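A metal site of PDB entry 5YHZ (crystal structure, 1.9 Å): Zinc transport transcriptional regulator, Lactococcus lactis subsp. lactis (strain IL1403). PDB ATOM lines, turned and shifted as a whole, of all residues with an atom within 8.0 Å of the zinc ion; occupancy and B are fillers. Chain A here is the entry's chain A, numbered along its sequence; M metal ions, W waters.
Three residues have an atom within 4 Å of the zinc ion: Cys 30, Glu 107 and His 111.
The zinc ion is bound by the side-chain carboxylate (OE2) of Glu 107, a ring nitrogen (NE2) of His 111, water W1 and the side-chain sulfur (SG) of Cys 30.
N of Glu 31 sits close to OE2 of Glu 107, 2.7 Å away.
OE1 of Glu 107 is in hydrogen-bond range of N of Ser 32.
The backbone carbonyl oxygen of Leu 27 lies within hydrogen-bond range of a ring nitrogen (ND1) of His 111, 2.7 Å away.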
ATOM      1  N   LYS A  22     -10.819  -8.188  31.457  1.00  0.00           N
ATOM      2  CA  LYS A  22     -10.010  -8.543  30.288  1.00  0.00           C
ATOM      3  C   LYS A  22     -10.725  -9.625  29.466  1.00  0.00           C
ATOM      4  O   LYS A  22     -11.618 -10.276  29.960  1.00  0.00           O
ATOM      5  CB  LYS A  22      -8.628  -9.072  30.724  1.00  0.00           C
ATOM      6  CG  LYS A  22      -7.903  -8.240  31.818  1.00  0.00           C
ATOM      7  CD  LYS A  22      -7.749  -6.768  31.444  1.00  0.00           C
ATOM      8  CE  LYS A  22      -6.680  -6.041  32.296  1.00  0.00           C
ATOM      9  NZ  LYS A  22      -5.231  -6.266  31.875  1.00  0.00           N
ATOM     10  N   LEU A  26      -4.144 -14.293  30.497  1.00  0.00           N
ATOM     11  CA  LEU A  26      -2.705 -14.200  30.355  1.00  0.00           C
ATOM     12  C   LEU A  26      -2.088 -14.296  31.729  1.00  0.00           C
ATOM     13  O   LEU A  26      -2.543 -13.627  32.637  1.00  0.00           O
ATOM     14  CB  LEU A  26      -2.367 -12.818  29.734  1.00  0.00           C
ATOM     15  CG  LEU A  26      -2.668 -12.716  28.256  1.00  0.00           C
ATOM     16  CD1 LEU A  26      -2.578 -11.238  27.721  1.00  0.00           C
ATOM     17  CD2 LEU A  26      -1.687 -13.558  27.531  1.00  0.00           C
ATOM     18  N   LEU A  27      -1.048 -15.123  31.866  1.00  0.00           N
ATOM     19  CA  LEU A  27      -0.325 -15.224  33.113  1.00  0.00           C
ATOM     20  C   LEU A  27       0.908 -14.272  33.025  1.00  0.00           C
ATOM     21  O   LEU A  27       1.261 -13.777  31.946  1.00  0.00           O
ATOM     22  CB  LEU A  27       0.124 -16.701  33.348  1.00  0.00           C
ATOM     23  CG  LEU A  27      -0.996 -17.756  33.425  1.00  0.00           C
ATOM     24  CD1 LEU A  27      -0.518 -19.252  33.443  1.00  0.00           C
ATOM     25  CD2 LEU A  27      -1.698 -17.439  34.702  1.00  0.00           C
ATOM     26  N   GLY A  28       1.584 -14.078  34.137  1.00  0.00           N
ATOM     27  CA  GLY A  28       2.799 -13.284  34.134  1.00  0.00           C
ATOM     28  C   GLY A  28       2.489 -11.967  34.783  1.00  0.00           C
ATOM     29  O   GLY A  28       1.405 -11.444  34.660  1.00  0.00           O
ATOM     30  N   LYS A  29       3.444 -11.463  35.565  1.00  0.00           N
ATOM     31  CA  LYS A  29       3.314 -10.176  36.207  1.00  0.00           C
ATOM     32  C   LYS A  29       3.064  -9.161  35.099  1.00  0.00           C
ATOM     33  O   LYS A  29       3.750  -9.182  34.073  1.00  0.00           O
ATOM     34  CB  LYS A  29       4.635  -9.848  36.934  1.00  0.00           C
ATOM     35  CG  LYS A  29       4.549  -8.724  37.943  1.00  0.00           C
ATOM     36  CD  LYS A  29       3.510  -8.971  39.016  1.00  0.00           C
ATOM     37  CE  LYS A  29       3.839  -8.104  40.244  1.00  0.00           C
ATOM     38  NZ  LYS A  29       4.317  -6.738  39.803  1.00  0.00           N
ATOM     39  N   CYS A  30       2.101  -8.278  35.307  1.00  0.00           N
ATOM     40  CA  CYS A  30       1.707  -7.302  34.302  1.00  0.00           C
ATOM     41  C   CYS A  30       1.920  -5.898  34.826  1.00  0.00           C
ATOM     42  O   CYS A  30       1.221  -5.478  35.741  1.00  0.00           O
ATOM     43  CB  CYS A  30       0.234  -7.484  33.952  1.00  0.00           C
ATOM     44  SG  CYS A  30      -0.344  -6.329  32.718  1.00  0.00           S
ATOM     45  N   GLU A  31       2.881  -5.177  34.231  1.00  0.00           N
ATOM     46  CA  GLU A  31       3.263  -3.821  34.655  1.00  0.00           C
ATOM     47  C   GLU A  31       2.555  -2.710  33.873  1.00  0.00           C
ATOM     48  O   GLU A  31       2.138  -1.687  34.440  1.00  0.00           O
ATOM     49  CB  GLU A  31       4.755  -3.641  34.446  1.00  0.00           C
ATOM     50  CG  GLU A  31       5.403  -2.790  35.506  1.00  0.00           C
ATOM     51  CD  GLU A  31       6.864  -3.119  35.648  1.00  0.00           C
ATOM     52  OE1 GLU A  31       7.688  -2.170  35.607  1.00  0.00           O
ATOM     53  OE2 GLU A  31       7.202  -4.328  35.808  1.00  0.00           O
ATOM     54  N   SER A  32       2.451  -2.919  32.570  1.00  0.00           N
ATOM     55  CA  SER A  32       1.863  -1.933  31.670  1.00  0.00           C
ATOM     56  C   SER A  32       0.475  -1.583  32.165  1.00  0.00           C
ATOM     57  O   SER A  32      -0.197  -2.373  32.833  1.00  0.00           O
ATOM     58  CB  SER A  32       1.816  -2.475  30.226  1.00  0.00           C
ATOM     59  OG  SER A  32       1.045  -1.656  29.365  1.00  0.00           O
ATOM     60  N   ASP A  33       0.048  -0.363  31.863  1.00  0.00           N
ATOM     61  CA  ASP A  33      -1.272   0.086  32.234  1.00  0.00           C
ATOM     62  C   ASP A  33      -2.009   0.442  30.941  1.00  0.00           C
ATOM     63  O   ASP A  33      -3.118   0.963  30.972  1.00  0.00           O
ATOM     64  CB  ASP A  33      -1.193   1.289  33.191  1.00  0.00           C
ATOM     65  CG  ASP A  33      -0.206   2.343  32.707  1.00  0.00           C
ATOM     66  OD1 ASP A  33       0.885   2.000  32.204  1.00  0.00           O
ATOM     67  OD2 ASP A  33      -0.534   3.545  32.845  1.00  0.00           O
ATOM     68  N   VAL A  34      -1.366   0.144  29.801  1.00  0.00           N
ATOM     69  CA  VAL A  34      -1.927   0.509  28.493  1.00  0.00           C
ATOM     70  C   VAL A  34      -3.108  -0.381  28.123  1.00  0.00           C
ATOM     71  O   VAL A  34      -2.927  -1.471  27.611  1.00  0.00           O
ATOM     72  CB  VAL A  34      -0.853   0.452  27.354  1.00  0.00           C
ATOM     73  CG1 VAL A  34      -1.502   0.727  25.997  1.00  0.00           C
ATOM     74  CG2 VAL A  34       0.309   1.437  27.607  1.00  0.00           C
ATOM     75  N   PRO A 103       7.841  -1.386  24.688  1.00  0.00           N
ATOM     76  CA  PRO A 103       7.758  -2.225  25.890  1.00  0.00           C
ATOM     77  C   PRO A 103       6.407  -2.866  26.044  1.00  0.00           C
ATOM     78  O   PRO A 103       6.255  -3.834  26.782  1.00  0.00           O
ATOM     79  CB  PRO A 103       8.009  -1.227  27.039  1.00  0.00           C
ATOM     80  CG  PRO A 103       7.679   0.106  26.467  1.00  0.00           C
ATOM     81  CD  PRO A 103       8.040   0.038  25.006  1.00  0.00           C
ATOM     82  N   VAL A 104       5.419  -2.334  25.361  1.00  0.00           N
ATOM     83  CA  VAL A 104       4.055  -2.790  25.541  1.00  0.00           C
ATOM     84  C   VAL A 104       3.933  -4.061  24.759  1.00  0.00           C
ATOM     85  O   VAL A 104       3.433  -5.055  25.300  1.00  0.00           O
ATOM     86  CB  VAL A 104       3.033  -1.782  25.034  1.00  0.00           C
ATOM     87  CG1 VAL A 104       1.585  -2.326  25.201  1.00  0.00           C
ATOM     88  CG2 VAL A 104       3.193  -0.449  25.768  1.00  0.00           C
ATOM     89  N   LYS A 106       6.496  -5.946  23.874  1.00  0.00           N
ATOM     90  CA  LYS A 106       7.427  -6.940  24.360  1.00  0.00           C
ATOM     91  C   LYS A 106       6.820  -7.565  25.619  1.00  0.00           C
ATOM     92  O   LYS A 106       7.013  -8.752  25.853  1.00  0.00           O
ATOM     93  CB  LYS A 106       8.789  -6.343  24.661  1.00  0.00           C
ATOM     94  CG  LYS A 106       9.624  -7.215  25.577  1.00  0.00           C
ATOM     95  CD  LYS A 106      11.086  -6.765  25.597  1.00  0.00           C
ATOM     96  CE  LYS A 106      11.948  -7.671  26.473  1.00  0.00           C
ATOM     97  NZ  LYS A 106      13.339  -7.113  26.628  1.00  0.00           N
ATOM     98  N   GLU A 107       6.045  -6.777  26.374  1.00  0.00           N
ATOM     99  CA  GLU A 107       5.395  -7.271  27.579  1.00  0.00           C
ATOM    100  C   GLU A 107       4.277  -8.235  27.244  1.00  0.00           C
ATOM    101  O   GLU A 107       4.130  -9.225  27.918  1.00  0.00           O
ATOM    102  CB  GLU A 107       4.755  -6.189  28.434  1.00  0.00           C
ATOM    103  CG  GLU A 107       4.127  -6.820  29.698  1.00  0.00           C
ATOM    104  CD  GLU A 107       3.731  -5.807  30.742  1.00  0.00           C
ATOM    105  OE1 GLU A 107       4.054  -4.612  30.596  1.00  0.00           O
ATOM    106  OE2 GLU A 107       3.111  -6.205  31.750  1.00  0.00           O
ATOM    107  N   HIS A 108       3.477  -7.909  26.237  1.00  0.00           N
ATOM    108  CA  HIS A 108       2.338  -8.753  25.913  1.00  0.00           C
ATOM    109  C   HIS A 108       2.849 -10.050  25.371  1.00  0.00           C
ATOM    110  O   HIS A 108       2.402 -11.137  25.775  1.00  0.00           O
ATOM    111  CB  HIS A 108       1.373  -8.035  24.974  1.00  0.00           C
ATOM    112  CG  HIS A 108       0.052  -8.708  24.833  1.00  0.00           C
ATOM    113  ND1 HIS A 108      -1.083  -8.239  25.444  1.00  0.00           N
ATOM    114  CD2 HIS A 108      -0.330  -9.824  24.144  1.00  0.00           C
ATOM    115  CE1 HIS A 108      -2.115  -9.000  25.128  1.00  0.00           C
ATOM    116  NE2 HIS A 108      -1.678  -9.962  24.342  1.00  0.00           N
ATOM    117  N   ALA A 109       3.877  -9.975  24.539  1.00  0.00           N
ATOM    118  CA  ALA A 109       4.515 -11.152  23.991  1.00  0.00           C
ATOM    119  C   ALA A 109       5.094 -12.029  25.094  1.00  0.00           C
ATOM    120  O   ALA A 109       5.163 -13.233  24.957  1.00  0.00           O
ATOM    121  CB  ALA A 109       5.603 -10.772  23.012  1.00  0.00           C
ATOM    122  N   THR A 110       5.594 -11.399  26.138  1.00  0.00           N
ATOM    123  CA  THR A 110       6.171 -12.121  27.254  1.00  0.00           C
ATOM    124  C   THR A 110       5.042 -12.812  28.007  1.00  0.00           C
ATOM    125  O   THR A 110       5.210 -13.903  28.514  1.00  0.00           O
ATOM    126  CB  THR A 110       6.843 -11.121  28.186  1.00  0.00           C
ATOM    127  OG1 THR A 110       8.042 -10.698  27.555  1.00  0.00           O
ATOM    128  CG2 THR A 110       7.143 -11.739  29.542  1.00  0.00           C
ATOM    129  N   HIS A 111       3.908 -12.150  28.112  1.00  0.00           N
ATOM    130  CA  HIS A 111       2.763 -12.842  28.680  1.00  0.00           C
ATOM    131  C   HIS A 111       2.419 -14.064  27.895  1.00  0.00           C
ATOM    132  O   HIS A 111       2.130 -15.120  28.453  1.00  0.00           O
ATOM    133  CB  HIS A 111       1.559 -11.943  28.685  1.00  0.00           C
ATOM    134  CG  HIS A 111       1.610 -10.923  29.755  1.00  0.00           C
ATOM    135  ND1 HIS A 111       1.669 -11.247  31.083  1.00  0.00           N
ATOM    136  CD2 HIS A 111       1.607  -9.571  29.690  1.00  0.00           C
ATOM    137  CE1 HIS A 111       1.698 -10.141  31.802  1.00  0.00           C
ATOM    138  NE2 HIS A 111       1.661  -9.115  30.979  1.00  0.00           N
HETATM  139 ZN    ZN M   1       1.161  -6.908  30.916  1.00  0.00          ZN
HETATM  140  O   HOH W   1       0.666  -6.281  28.752  1.00  0.00           O
